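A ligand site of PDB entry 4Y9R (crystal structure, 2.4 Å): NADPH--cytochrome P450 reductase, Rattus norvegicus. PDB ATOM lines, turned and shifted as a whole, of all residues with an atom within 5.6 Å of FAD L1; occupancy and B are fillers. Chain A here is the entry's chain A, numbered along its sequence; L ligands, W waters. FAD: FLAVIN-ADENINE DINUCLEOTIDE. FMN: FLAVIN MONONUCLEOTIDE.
N of Ser 400 lies within hydrogen-bond range of O4 of FAD L1 (3.1 Å).
The backbone NH (N) of Thr 434 is in hydrogen-bond range of an oxygen (O1P) of FAD L1.
An oxygen (O1A) of FAD L1 lies within hydrogen-bond range of the backbone NH (N) of Val 432 (3.0 Å).
The side-chain hydroxyl (OG1) of Thr 434 lies within hydrogen-bond range of an oxygen (O1P) of FAD L1, at 2.9 Å.
The backbone NH (N) of Val 417 is in hydrogen-bond range of an oxygen (O2) of FAD L1 (3.3 Å).
An oxygen (O2') of FAD L1 sits at hydrogen-bond distance from the backbone NH (N) of Tyr 398.
A nitrogen (N3) of FAD L1 sits at hydrogen-bond distance from the backbone carbonyl oxygen of Cys 415 (2.8 Å).
O2B of FAD L1 sits at hydrogen-bond distance from NH2 of Arg 367 (3.4 Å).
OH of Tyr 399 sits at hydrogen-bond distance from O4' of FAD L1 (2.8 Å).
NE of Arg 397 lies within salt-bridge range of O2P of FAD L1 (2.8 Å).
The backbone carbonyl oxygen of Tyr 398 lies within hydrogen-bond range of an oxygen (O2') of FAD L1, at 2.8 Å.
O2P of FAD L1 lies within hydrogen-bond range of N of Ala 433, at 2.8 Å.
The side-chain hydroxyl of Thr 434 sits at hydrogen-bond distance from the backbone NH of Val 419.
A ring nitrogen (NE2) of His 262 sits at hydrogen-bond distance from the side-chain carboxylate of Asp 618.
The backbone carbonyl oxygen (O) of His 262 lies within hydrogen-bond range of the backbone NH (N) of Arg 457 (2.9 Å).
The side-chain hydroxyl (OG) of Ser 400 is in hydrogen-bond range of the side-chain carboxylate (OD2) of Asp 618, at 2.6 Å.
N of Gly 431 is in hydrogen-bond range of O of Val 419, 2.9 Å away.
The guanidinium group of Arg 367 is in hydrogen-bond range of the side-chain amide oxygen of Asn 322 (3.1 Å).
The backbone carbonyl oxygen (O) of Gly 431 is in hydrogen-bond range of the side-chain hydroxyl (OG) of Ser 435.
OH of Tyr 421 sits at hydrogen-bond distance from NE of Arg 367, at 3.3 Å.
His 262 touches FAD L1 (NE2 to C7M, 3.7 Å).
CA of Ala 416 touches O2 of FAD L1, at 3.2 Å.
Val 419 touches FAD L1.
Tyr 421 touches FAD L1.
Gly 431 touches FAD L1.
Arg 457 touches FAD L1.
CG2 of Thr 478 touches O2 of FAD L1, at 3.9 Å.
Ala 481 touches FAD L1 (CB to O4, 3.8 Å).
CE3 of Trp 620 touches C5X of FAD L1, at 3.3 Å.
Hydrophobic or aromatic side chains within 4 Å of FAD L1: His 262, Tyr 399, Ala 416, Val 417, Val 419, Tyr 421, Val 432, Ala 433, Ala 481 and Trp 620.
Within 4 Å of FAD L1: His 262, Arg 367, Arg 397, Tyr 398, Tyr 399, Ser 400, Cys 415, Ala 416, Val 417, Val 419, Tyr 421, Gly 431, Val 432, Ala 433, Thr 434, Arg 457, Thr 478, Ala 481 and Trp 620.
The nearest printed residue that does not touch FAD L1 is Asp 618 (4.2 Å).
Water W7 lies within hydrogen-bond range of an oxygen (O4) of FAD L1, the backbone NH of Cys 415 and the backbone carbonyl oxygen of Ser 400.
Water W2 bridges O4' of FAD L1 (2.7 Å) and O of Val 417 (3.0 Å).
Water W4 bridges O2' of FAD L1 (2.7 Å) and N of Tyr 398 (2.9 Å).
Water W3 bridges O of Lys 430 and O1A of FAD L1.
Water W5 lies within hydrogen-bond range of OH of Tyr 421 (2.6 Å), O4B of FAD L1 (3.0 Å) and NH1 of Arg 367 (3.2 Å).
Water W8 lies within hydrogen-bond range of O3' of FAD L1 (3.1 Å) and O of Ser 621 (3.4 Å).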
ATOM      1  N   HIS A 262      11.696 -40.079 -14.931  1.00  0.00           N
ATOM      2  CA  HIS A 262      11.542 -39.294 -16.142  1.00  0.00           C
ATOM      3  C   HIS A 262      12.422 -39.865 -17.257  1.00  0.00           C
ATOM      4  O   HIS A 262      13.480 -40.433 -16.987  1.00  0.00           O
ATOM      5  CB  HIS A 262      11.958 -37.848 -15.896  1.00  0.00           C
ATOM      6  CG  HIS A 262      11.163 -37.137 -14.840  1.00  0.00           C
ATOM      7  ND1 HIS A 262      11.694 -36.787 -13.618  1.00  0.00           N
ATOM      8  CD2 HIS A 262       9.868 -36.750 -14.812  1.00  0.00           C
ATOM      9  CE1 HIS A 262      10.764 -36.206 -12.890  1.00  0.00           C
ATOM     10  NE2 HIS A 262       9.642 -36.176 -13.587  1.00  0.00           N
ATOM     11  N   THR A 321      15.118 -21.950 -31.590  1.00  0.00           N
ATOM     12  CA  THR A 321      13.720 -21.605 -31.397  1.00  0.00           C
ATOM     13  C   THR A 321      13.389 -20.737 -30.198  1.00  0.00           C
ATOM     14  O   THR A 321      12.430 -19.972 -30.231  1.00  0.00           O
ATOM     15  CB  THR A 321      12.879 -22.881 -31.331  1.00  0.00           C
ATOM     16  OG1 THR A 321      13.448 -23.766 -30.363  1.00  0.00           O
ATOM     17  CG2 THR A 321      12.855 -23.582 -32.683  1.00  0.00           C
ATOM     18  N   ASN A 322      14.132 -20.869 -29.109  1.00  0.00           N
ATOM     19  CA  ASN A 322      13.837 -20.025 -27.965  1.00  0.00           C
ATOM     20  C   ASN A 322      14.342 -18.625 -28.244  1.00  0.00           C
ATOM     21  O   ASN A 322      15.308 -18.449 -28.992  1.00  0.00           O
ATOM     22  CB  ASN A 322      14.475 -20.602 -26.696  1.00  0.00           C
ATOM     23  CG  ASN A 322      13.682 -21.773 -26.147  1.00  0.00           C
ATOM     24  OD1 ASN A 322      12.451 -21.705 -26.106  1.00  0.00           O
ATOM     25  ND2 ASN A 322      14.371 -22.834 -25.731  1.00  0.00           N
ATOM     26  N   ARG A 367       7.921 -13.975 -28.635  1.00  0.00           N
ATOM     27  CA  ARG A 367       8.575 -15.251 -28.870  1.00  0.00           C
ATOM     28  C   ARG A 367       9.227 -15.312 -30.245  1.00  0.00           C
ATOM     29  O   ARG A 367       9.032 -16.283 -30.990  1.00  0.00           O
ATOM     30  CB  ARG A 367       7.575 -16.392 -28.731  1.00  0.00           C
ATOM     31  CG  ARG A 367       6.908 -16.512 -27.364  1.00  0.00           C
ATOM     32  CD  ARG A 367       7.861 -17.102 -26.339  1.00  0.00           C
ATOM     33  NE  ARG A 367       8.486 -18.326 -26.845  1.00  0.00           N
ATOM     34  CZ  ARG A 367       9.404 -19.042 -26.188  1.00  0.00           C
ATOM     35  NH1 ARG A 367       9.884 -20.149 -26.754  1.00  0.00           N
ATOM     36  NH2 ARG A 367       9.833 -18.665 -24.992  1.00  0.00           N
ATOM     37  N   ARG A 397      14.519 -32.850 -23.627  1.00  0.00           N
ATOM     38  CA  ARG A 397      13.257 -32.547 -22.989  1.00  0.00           C
ATOM     39  C   ARG A 397      12.941 -33.758 -22.107  1.00  0.00           C
ATOM     40  O   ARG A 397      13.293 -34.880 -22.461  1.00  0.00           O
ATOM     41  CB  ARG A 397      12.156 -32.361 -24.036  1.00  0.00           C
ATOM     42  CG  ARG A 397      12.003 -30.958 -24.591  1.00  0.00           C
ATOM     43  CD  ARG A 397      13.230 -30.431 -25.298  1.00  0.00           C
ATOM     44  NE  ARG A 397      12.923 -29.147 -25.926  1.00  0.00           N
ATOM     45  CZ  ARG A 397      13.822 -28.288 -26.412  1.00  0.00           C
ATOM     46  NH1 ARG A 397      13.399 -27.154 -26.953  1.00  0.00           N
ATOM     47  NH2 ARG A 397      15.122 -28.540 -26.340  1.00  0.00           N
ATOM     48  N   TYR A 398      12.306 -33.543 -20.967  1.00  0.00           N
ATOM     49  CA  TYR A 398      11.966 -34.634 -20.066  1.00  0.00           C
ATOM     50  C   TYR A 398      10.487 -34.950 -20.116  1.00  0.00           C
ATOM     51  O   TYR A 398       9.657 -34.066 -20.353  1.00  0.00           O
ATOM     52  CB  TYR A 398      12.363 -34.282 -18.632  1.00  0.00           C
ATOM     53  CG  TYR A 398      13.861 -34.212 -18.406  1.00  0.00           C
ATOM     54  CD1 TYR A 398      14.605 -35.368 -18.182  1.00  0.00           C
ATOM     55  CD2 TYR A 398      14.524 -32.985 -18.437  1.00  0.00           C
ATOM     56  CE1 TYR A 398      15.988 -35.306 -17.999  1.00  0.00           C
ATOM     57  CE2 TYR A 398      15.910 -32.909 -18.256  1.00  0.00           C
ATOM     58  CZ  TYR A 398      16.638 -34.084 -18.035  1.00  0.00           C
ATOM     59  OH  TYR A 398      18.001 -34.016 -17.849  1.00  0.00           O
ATOM     60  N   TYR A 399      10.145 -36.209 -19.875  1.00  0.00           N
ATOM     61  CA  TYR A 399       8.748 -36.625 -19.885  1.00  0.00           C
ATOM     62  C   TYR A 399       8.537 -37.649 -18.773  1.00  0.00           C
ATOM     63  O   TYR A 399       9.368 -38.514 -18.560  1.00  0.00           O
ATOM     64  CB  TYR A 399       8.407 -37.202 -21.266  1.00  0.00           C
ATOM     65  CG  TYR A 399       8.479 -36.158 -22.360  1.00  0.00           C
ATOM     66  CD1 TYR A 399       7.373 -35.350 -22.657  1.00  0.00           C
ATOM     67  CD2 TYR A 399       9.655 -35.935 -23.077  1.00  0.00           C
ATOM     68  CE1 TYR A 399       7.444 -34.344 -23.626  1.00  0.00           C
ATOM     69  CE2 TYR A 399       9.732 -34.932 -24.061  1.00  0.00           C
ATOM     70  CZ  TYR A 399       8.618 -34.140 -24.320  1.00  0.00           C
ATOM     71  OH  TYR A 399       8.673 -33.157 -25.270  1.00  0.00           O
ATOM     72  N   SER A 400       7.436 -37.523 -18.047  1.00  0.00           N
ATOM     73  CA  SER A 400       7.154 -38.456 -16.957  1.00  0.00           C
ATOM     74  C   SER A 400       6.786 -39.791 -17.563  1.00  0.00           C
ATOM     75  O   SER A 400       5.759 -39.906 -18.255  1.00  0.00           O
ATOM     76  CB  SER A 400       5.992 -37.942 -16.096  1.00  0.00           C
ATOM     77  OG  SER A 400       6.257 -36.641 -15.606  1.00  0.00           O
ATOM     78  N   CYS A 415       3.510 -39.603 -22.612  1.00  0.00           N
ATOM     79  CA  CYS A 415       2.207 -38.985 -22.797  1.00  0.00           C
ATOM     80  C   CYS A 415       2.455 -37.502 -22.926  1.00  0.00           C
ATOM     81  O   CYS A 415       2.768 -36.834 -21.941  1.00  0.00           O
ATOM     82  CB  CYS A 415       1.312 -39.249 -21.582  1.00  0.00           C
ATOM     83  SG  CYS A 415      -0.230 -38.329 -21.590  1.00  0.00           S
ATOM     84  N   ALA A 416       2.312 -36.964 -24.132  1.00  0.00           N
ATOM     85  CA  ALA A 416       2.599 -35.559 -24.335  1.00  0.00           C
ATOM     86  C   ALA A 416       1.632 -34.816 -25.208  1.00  0.00           C
ATOM     87  O   ALA A 416       0.985 -35.391 -26.080  1.00  0.00           O
ATOM     88  CB  ALA A 416       3.992 -35.428 -24.914  1.00  0.00           C
ATOM     89  N   VAL A 417       1.559 -33.519 -24.958  1.00  0.00           N
ATOM     90  CA  VAL A 417       0.728 -32.644 -25.762  1.00  0.00           C
ATOM     91  C   VAL A 417       1.695 -31.991 -26.739  1.00  0.00           C
ATOM     92  O   VAL A 417       2.783 -31.549 -26.343  1.00  0.00           O
ATOM     93  CB  VAL A 417       0.010 -31.547 -24.886  1.00  0.00           C
ATOM     94  CG1 VAL A 417       0.988 -30.908 -23.920  1.00  0.00           C
ATOM     95  CG2 VAL A 417      -0.613 -30.485 -25.804  1.00  0.00           C
ATOM     96  N   VAL A 419       3.123 -29.142 -28.822  1.00  0.00           N
ATOM     97  CA  VAL A 419       3.108 -27.708 -28.663  1.00  0.00           C
ATOM     98  C   VAL A 419       3.103 -27.018 -30.018  1.00  0.00           C
ATOM     99  O   VAL A 419       3.941 -27.276 -30.876  1.00  0.00           O
ATOM    100  CB  VAL A 419       4.314 -27.216 -27.838  1.00  0.00           C
ATOM    101  CG1 VAL A 419       4.352 -25.697 -27.772  1.00  0.00           C
ATOM    102  CG2 VAL A 419       4.248 -27.821 -26.431  1.00  0.00           C
ATOM    103  N   TYR A 421       1.511 -22.991 -31.162  1.00  0.00           N
ATOM    104  CA  TYR A 421       0.691 -21.840 -30.810  1.00  0.00           C
ATOM    105  C   TYR A 421       0.941 -20.626 -31.709  1.00  0.00           C
ATOM    106  O   TYR A 421       1.967 -20.540 -32.383  1.00  0.00           O
ATOM    107  CB  TYR A 421       0.961 -21.421 -29.371  1.00  0.00           C
ATOM    108  CG  TYR A 421       2.415 -21.091 -29.116  1.00  0.00           C
ATOM    109  CD1 TYR A 421       3.349 -22.098 -28.855  1.00  0.00           C
ATOM    110  CD2 TYR A 421       2.879 -19.767 -29.188  1.00  0.00           C
ATOM    111  CE1 TYR A 421       4.697 -21.804 -28.665  1.00  0.00           C
ATOM    112  CE2 TYR A 421       4.227 -19.467 -29.005  1.00  0.00           C
ATOM    113  CZ  TYR A 421       5.128 -20.485 -28.731  1.00  0.00           C
ATOM    114  OH  TYR A 421       6.467 -20.206 -28.567  1.00  0.00           O
ATOM    115  N   GLU A 422      -0.006 -19.705 -31.703  1.00  0.00           N
ATOM    116  CA  GLU A 422       0.120 -18.480 -32.486  1.00  0.00           C
ATOM    117  C   GLU A 422       0.923 -17.534 -31.605  1.00  0.00           C
ATOM    118  O   GLU A 422       0.493 -17.181 -30.503  1.00  0.00           O
ATOM    119  CB  GLU A 422      -1.262 -17.864 -32.757  1.00  0.00           C
ATOM    120  CG  GLU A 422      -2.314 -18.867 -33.185  1.00  0.00           C
ATOM    121  CD  GLU A 422      -3.721 -18.260 -33.272  1.00  0.00           C
ATOM    122  OE1 GLU A 422      -4.180 -17.673 -32.263  1.00  0.00           O
ATOM    123  OE2 GLU A 422      -4.361 -18.393 -34.335  1.00  0.00           O
ATOM    124  N   LYS A 430       6.398 -23.915 -33.241  1.00  0.00           N
ATOM    125  CA  LYS A 430       6.296 -25.355 -33.013  1.00  0.00           C
ATOM    126  C   LYS A 430       7.285 -25.823 -31.936  1.00  0.00           C
ATOM    127  O   LYS A 430       8.447 -25.439 -31.947  1.00  0.00           O
ATOM    128  CB  LYS A 430       6.602 -26.114 -34.307  1.00  0.00           C
ATOM    129  CG  LYS A 430       5.789 -25.689 -35.522  1.00  0.00           C
ATOM    130  CD  LYS A 430       4.398 -26.286 -35.486  1.00  0.00           C
ATOM    131  CE  LYS A 430       4.443 -27.807 -35.560  1.00  0.00           C
ATOM    132  NZ  LYS A 430       4.917 -28.314 -36.878  1.00  0.00           N
ATOM    133  N   GLY A 431       6.812 -26.661 -31.018  1.00  0.00           N
ATOM    134  CA  GLY A 431       7.683 -27.188 -29.974  1.00  0.00           C
ATOM    135  C   GLY A 431       8.690 -28.134 -30.594  1.00  0.00           C
ATOM    136  O   GLY A 431       8.329 -29.052 -31.348  1.00  0.00           O
ATOM    137  N   VAL A 432       9.967 -27.932 -30.278  1.00  0.00           N
ATOM    138  CA  VAL A 432      11.018 -28.759 -30.848  1.00  0.00           C
ATOM    139  C   VAL A 432      10.839 -30.261 -30.652  1.00  0.00           C
ATOM    140  O   VAL A 432      10.759 -31.008 -31.618  1.00  0.00           O
ATOM    141  CB  VAL A 432      12.407 -28.362 -30.282  1.00  0.00           C
ATOM    142  CG1 VAL A 432      13.500 -29.205 -30.953  1.00  0.00           C
ATOM    143  CG2 VAL A 432      12.655 -26.861 -30.512  1.00  0.00           C
ATOM    144  N   ALA A 433      10.755 -30.700 -29.395  1.00  0.00           N
ATOM    145  CA  ALA A 433      10.619 -32.115 -29.097  1.00  0.00           C
ATOM    146  C   ALA A 433       9.301 -32.752 -29.504  1.00  0.00           C
ATOM    147  O   ALA A 433       9.280 -33.829 -30.088  1.00  0.00           O
ATOM    148  CB  ALA A 433      10.882 -32.377 -27.611  1.00  0.00           C
ATOM    149  N   THR A 434       8.187 -32.103 -29.178  1.00  0.00           N
ATOM    150  CA  THR A 434       6.914 -32.700 -29.510  1.00  0.00           C
ATOM    151  C   THR A 434       6.638 -32.754 -31.011  1.00  0.00           C
ATOM    152  O   THR A 434       6.055 -33.725 -31.477  1.00  0.00           O
ATOM    153  CB  THR A 434       5.760 -31.994 -28.763  1.00  0.00           C
ATOM    154  OG1 THR A 434       5.673 -30.630 -29.162  1.00  0.00           O
ATOM    155  CG2 THR A 434       6.004 -32.079 -27.262  1.00  0.00           C
ATOM    156  N   SER A 435       7.070 -31.748 -31.780  1.00  0.00           N
ATOM    157  CA  SER A 435       6.839 -31.787 -33.226  1.00  0.00           C
ATOM    158  C   SER A 435       7.576 -33.009 -33.760  1.00  0.00           C
ATOM    159  O   SER A 435       7.051 -33.774 -34.572  1.00  0.00           O
ATOM    160  CB  SER A 435       7.386 -30.540 -33.929  1.00  0.00           C
ATOM    161  OG  SER A 435       6.723 -29.360 -33.514  1.00  0.00           O
ATOM    162  N   ARG A 457      16.188 -40.692 -16.070  1.00  0.00           N
ATOM    163  CA  ARG A 457      16.685 -39.913 -14.938  1.00  0.00           C
ATOM    164  C   ARG A 457      15.819 -40.301 -13.771  1.00  0.00           C
ATOM    165  O   ARG A 457      14.608 -40.159 -13.810  1.00  0.00           O
ATOM    166  CB  ARG A 457      16.563 -38.404 -15.180  1.00  0.00           C
ATOM    167  CG  ARG A 457      17.189 -37.593 -14.037  1.00  0.00           C
ATOM    168  CD  ARG A 457      16.992 -36.098 -14.193  1.00  0.00           C
ATOM    169  NE  ARG A 457      15.589 -35.718 -14.037  1.00  0.00           N
ATOM    170  CZ  ARG A 457      15.092 -34.525 -14.366  1.00  0.00           C
ATOM    171  NH1 ARG A 457      15.894 -33.589 -14.874  1.00  0.00           N
ATOM    172  NH2 ARG A 457      13.799 -34.271 -14.201  1.00  0.00           N
ATOM    173  N   THR A 478      -2.195 -33.623 -19.011  1.00  0.00           N
ATOM    174  CA  THR A 478      -1.050 -34.506 -19.163  1.00  0.00           C
ATOM    175  C   THR A 478      -0.516 -34.918 -17.805  1.00  0.00           C
ATOM    176  O   THR A 478       0.368 -35.752 -17.718  1.00  0.00           O
ATOM    177  CB  THR A 478       0.088 -33.863 -19.990  1.00  0.00           C
ATOM    178  OG1 THR A 478       0.429 -32.591 -19.426  1.00  0.00           O
ATOM    179  CG2 THR A 478      -0.338 -33.676 -21.435  1.00  0.00           C
ATOM    180  N   ALA A 481       0.129 -38.730 -16.903  1.00  0.00           N
ATOM    181  CA  ALA A 481       1.278 -39.531 -17.313  1.00  0.00           C
ATOM    182  C   ALA A 481       1.873 -40.524 -16.315  1.00  0.00           C
ATOM    183  O   ALA A 481       1.789 -41.735 -16.520  1.00  0.00           O
ATOM    184  CB  ALA A 481       2.379 -38.609 -17.846  1.00  0.00           C
ATOM    185  N   ASP A 618       5.268 -33.523  -9.207  1.00  0.00           N
ATOM    186  CA  ASP A 618       5.883 -33.757 -10.494  1.00  0.00           C
ATOM    187  C   ASP A 618       5.140 -32.815 -11.405  1.00  0.00           C
ATOM    188  O   ASP A 618       4.255 -33.216 -12.178  1.00  0.00           O
ATOM    189  CB  ASP A 618       5.714 -35.202 -10.980  1.00  0.00           C
ATOM    190  CG  ASP A 618       6.275 -35.411 -12.381  1.00  0.00           C
ATOM    191  OD1 ASP A 618       7.202 -34.665 -12.750  1.00  0.00           O
ATOM    192  OD2 ASP A 618       5.800 -36.300 -13.108  1.00  0.00           O
ATOM    193  N   VAL A 619       5.473 -31.543 -11.271  1.00  0.00           N
ATOM    194  CA  VAL A 619       4.842 -30.485 -12.035  1.00  0.00           C
ATOM    195  C   VAL A 619       5.864 -29.734 -12.862  1.00  0.00           C
ATOM    196  O   VAL A 619       7.071 -29.806 -12.596  1.00  0.00           O
ATOM    197  CB  VAL A 619       4.102 -29.535 -11.089  1.00  0.00           C
ATOM    198  CG1 VAL A 619       3.033 -30.295 -10.340  1.00  0.00           C
ATOM    199  CG2 VAL A 619       5.086 -28.931 -10.087  1.00  0.00           C
ATOM    200  N   TRP A 620       5.390 -29.005 -13.860  1.00  0.00           N
ATOM    201  CA  TRP A 620       6.269 -28.248 -14.732  1.00  0.00           C
ATOM    202  C   TRP A 620       5.451 -27.157 -15.407  1.00  0.00           C
ATOM    203  O   TRP A 620       4.253 -27.030 -15.145  1.00  0.00           O
ATOM    204  CB  TRP A 620       6.869 -29.184 -15.783  1.00  0.00           C
ATOM    205  CG  TRP A 620       5.833 -29.861 -16.643  1.00  0.00           C
ATOM    206  CD1 TRP A 620       5.248 -29.365 -17.766  1.00  0.00           C
ATOM    207  CD2 TRP A 620       5.235 -31.153 -16.425  1.00  0.00           C
ATOM    208  NE1 TRP A 620       4.315 -30.253 -18.258  1.00  0.00           N
ATOM    209  CE2 TRP A 620       4.292 -31.358 -17.458  1.00  0.00           C
ATOM    210  CE3 TRP A 620       5.399 -32.158 -15.448  1.00  0.00           C
ATOM    211  CZ2 TRP A 620       3.511 -32.527 -17.545  1.00  0.00           C
ATOM    212  CZ3 TRP A 620       4.627 -33.324 -15.544  1.00  0.00           C
ATOM    213  CH2 TRP A 620       3.697 -33.489 -16.582  1.00  0.00           C
ATOM    214  N   SER A 621       6.095 -26.376 -16.267  1.00  0.00           N
ATOM    215  CA  SER A 621       5.431 -25.287 -16.970  1.00  0.00           C
ATOM    216  C   SER A 621       5.767 -25.315 -18.462  1.00  0.00           C
ATOM    217  O   SER A 621       6.480 -26.253 -18.893  1.00  0.00           O
ATOM    218  CB  SER A 621       5.840 -23.949 -16.371  1.00  0.00           C
ATOM    219  OG  SER A 621       5.558 -23.896 -14.983  1.00  0.00           O
ATOM    220  OXT SER A 621       5.322 -24.395 -19.196  1.00  0.00           O
HETATM  221  PA  FAD L   1       9.715 -26.216 -26.764  1.00  0.00           P
HETATM  222  O1A FAD L   1      10.296 -25.942 -28.102  1.00  0.00           O
HETATM  223  O2A FAD L   1      10.610 -26.625 -25.659  1.00  0.00           O
HETATM  224  O5B FAD L   1       8.868 -24.928 -26.315  1.00  0.00           O
HETATM  225  C5B FAD L   1       8.426 -24.788 -24.960  1.00  0.00           C
HETATM  226  C4B FAD L   1       8.081 -23.321 -24.684  1.00  0.00           C
HETATM  227  O4B FAD L   1       7.082 -22.839 -25.594  1.00  0.00           O
HETATM  228  C3B FAD L   1       7.387 -23.164 -23.350  1.00  0.00           C
HETATM  229  O3B FAD L   1       8.358 -23.224 -22.300  1.00  0.00           O
HETATM  230  C2B FAD L   1       6.895 -21.739 -23.498  1.00  0.00           C
HETATM  231  O2B FAD L   1       7.960 -20.822 -23.218  1.00  0.00           O
HETATM  232  C1B FAD L   1       6.513 -21.671 -24.973  1.00  0.00           C
HETATM  233  N9A FAD L   1       5.051 -21.748 -25.162  1.00  0.00           N
HETATM  234  C8A FAD L   1       4.230 -22.974 -25.130  1.00  0.00           C
HETATM  235  N7A FAD L   1       2.907 -22.422 -25.503  1.00  0.00           N
HETATM  236  C5A FAD L   1       3.004 -21.101 -25.609  1.00  0.00           C
HETATM  237  C6A FAD L   1       2.070 -20.210 -25.913  1.00  0.00           C
HETATM  238  N6A FAD L   1       0.853 -20.703 -26.167  1.00  0.00           N
HETATM  239  N1A FAD L   1       2.312 -18.889 -25.981  1.00  0.00           N
HETATM  240  C2A FAD L   1       3.603 -18.438 -25.716  1.00  0.00           C
HETATM  241  N3A FAD L   1       4.573 -19.396 -25.387  1.00  0.00           N
HETATM  242  C4A FAD L   1       4.249 -20.696 -25.348  1.00  0.00           C
HETATM  243  N1  FAD L   1       5.212 -32.541 -21.044  1.00  0.00           N
HETATM  244  C2  FAD L   1       4.256 -33.493 -21.435  1.00  0.00           C
HETATM  245  O2  FAD L   1       3.455 -33.236 -22.333  1.00  0.00           O
HETATM  246  N3  FAD L   1       4.158 -34.690 -20.731  1.00  0.00           N
HETATM  247  C4  FAD L   1       4.994 -34.936 -19.639  1.00  0.00           C
HETATM  248  O4  FAD L   1       4.945 -36.036 -19.072  1.00  0.00           O
HETATM  249  C4X FAD L   1       5.929 -33.985 -19.251  1.00  0.00           C
HETATM  250  N5  FAD L   1       6.608 -34.151 -18.106  1.00  0.00           N
HETATM  251  C5X FAD L   1       7.519 -33.232 -17.734  1.00  0.00           C
HETATM  252  C6  FAD L   1       8.301 -33.467 -16.611  1.00  0.00           C
HETATM  253  C7  FAD L   1       9.340 -32.590 -16.288  1.00  0.00           C
HETATM  254  C7M FAD L   1      10.213 -32.926 -15.255  1.00  0.00           C
HETATM  255  C8  FAD L   1       9.577 -31.479 -17.078  1.00  0.00           C
HETATM  256  C8M FAD L   1      10.575 -30.573 -16.735  1.00  0.00           C
HETATM  257  C9  FAD L   1       8.783 -31.248 -18.206  1.00  0.00           C
HETATM  258  C9A FAD L   1       7.764 -32.125 -18.539  1.00  0.00           C
HETATM  259  N10 FAD L   1       7.040 -31.944 -19.662  1.00  0.00           N
HETATM  260  C10 FAD L   1       6.029 -32.787 -19.941  1.00  0.00           C
HETATM  261  C1' FAD L   1       7.278 -30.784 -20.541  1.00  0.00           C
HETATM  262  C2' FAD L   1       8.329 -31.138 -21.592  1.00  0.00           C
HETATM  263  O2' FAD L   1       9.592 -31.340 -20.947  1.00  0.00           O
HETATM  264  C3' FAD L   1       8.475 -30.045 -22.651  1.00  0.00           C
HETATM  265  O3' FAD L   1       8.718 -28.776 -22.033  1.00  0.00           O
HETATM  266  C4' FAD L   1       7.201 -29.974 -23.510  1.00  0.00           C
HETATM  267  O4' FAD L   1       6.950 -31.239 -24.113  1.00  0.00           O
HETATM  268  C5' FAD L   1       7.431 -28.924 -24.611  1.00  0.00           C
HETATM  269  O5' FAD L   1       8.688 -29.187 -25.229  1.00  0.00           O
HETATM  270  P   FAD L   1       8.925 -28.907 -26.800  1.00  0.00           P
HETATM  271  O1P FAD L   1       7.920 -29.666 -27.582  1.00  0.00           O
HETATM  272  O2P FAD L   1      10.356 -29.125 -27.092  1.00  0.00           O
HETATM  273  O3P FAD L   1       8.576 -27.336 -26.932  1.00  0.00           O
HETATM  274  N1  FMN L   2      13.590 -22.749  -8.834  1.00  0.00           N
HETATM  275  C2  FMN L   2      13.662 -22.544  -7.498  1.00  0.00           C
HETATM  276  O2  FMN L   2      13.903 -21.415  -7.022  1.00  0.00           O
HETATM  277  N3  FMN L   2      13.440 -23.643  -6.697  1.00  0.00           N
HETATM  278  C4  FMN L   2      13.146 -24.949  -7.103  1.00  0.00           C
HETATM  279  O4  FMN L   2      12.990 -25.752  -6.195  1.00  0.00           O
HETATM  280  C4A FMN L   2      13.070 -25.174  -8.495  1.00  0.00           C
HETATM  281  N5  FMN L   2      12.767 -26.494  -8.927  1.00  0.00           N
HETATM  282  C5A FMN L   2      12.717 -26.631 -10.321  1.00  0.00           C
HETATM  283  C6  FMN L   2      12.406 -27.960 -10.787  1.00  0.00           C
HETATM  284  C7  FMN L   2      12.320 -28.249 -12.181  1.00  0.00           C
HETATM  285  C7M FMN L   2      11.984 -29.722 -12.534  1.00  0.00           C
HETATM  286  C8  FMN L   2      12.542 -27.166 -13.204  1.00  0.00           C
HETATM  287  C8M FMN L   2      12.487 -27.329 -14.581  1.00  0.00           C
HETATM  288  C9  FMN L   2      12.836 -25.885 -12.753  1.00  0.00           C
HETATM  289  C9A FMN L   2      12.937 -25.567 -11.321  1.00  0.00           C
HETATM  290  N10 FMN L   2      13.244 -24.227 -10.768  1.00  0.00           N
HETATM  291  C10 FMN L   2      13.304 -24.021  -9.315  1.00  0.00           C
HETATM  292  C1' FMN L   2      13.481 -23.122 -11.680  1.00  0.00           C
HETATM  293  C2' FMN L   2      14.982 -23.010 -12.083  1.00  0.00           C
HETATM  294  O2' FMN L   2      15.765 -22.744 -10.844  1.00  0.00           O
HETATM  295  C3' FMN L   2      15.211 -21.888 -13.073  1.00  0.00           C
HETATM  296  O3' FMN L   2      14.432 -22.208 -14.252  1.00  0.00           O
HETATM  297  C4' FMN L   2      16.749 -21.825 -13.422  1.00  0.00           C
HETATM  298  O4' FMN L   2      16.793 -20.694 -14.329  1.00  0.00           O
HETATM  299  C5' FMN L   2      17.257 -23.038 -14.203  1.00  0.00           C
HETATM  300  O5' FMN L   2      18.714 -22.953 -14.503  1.00  0.00           O
HETATM  301  P   FMN L   2      19.576 -23.996 -15.308  1.00  0.00           P
HETATM  302  O1P FMN L   2      19.166 -24.011 -16.736  1.00  0.00           O
HETATM  303  O2P FMN L   2      19.492 -25.299 -14.456  1.00  0.00           O
HETATM  304  O3P FMN L   2      21.017 -23.304 -15.221  1.00  0.00           O
HETATM  305  O   HOH W   1      12.446 -24.627 -24.559  1.00  0.00           O
HETATM  306  O   HOH W   2       4.295 -31.140 -23.842  1.00  0.00           O
HETATM  307  O   HOH W   3       9.396 -23.858 -30.070  1.00  0.00           O
HETATM  308  O   HOH W   4      12.218 -30.672 -20.493  1.00  0.00           O
HETATM  309  O   HOH W   5       8.102 -22.175 -28.381  1.00  0.00           O
HETATM  310  O   HOH W   6      10.668 -27.608 -23.383  1.00  0.00           O
HETATM  311  O   HOH W   7       4.942 -38.231 -20.503  1.00  0.00           O
HETATM  312  O   HOH W   8       9.452 -27.976 -19.130  1.00  0.00           O
HETATM  313  O   HOH W   9      11.854 -23.580 -28.196  1.00  0.00           O
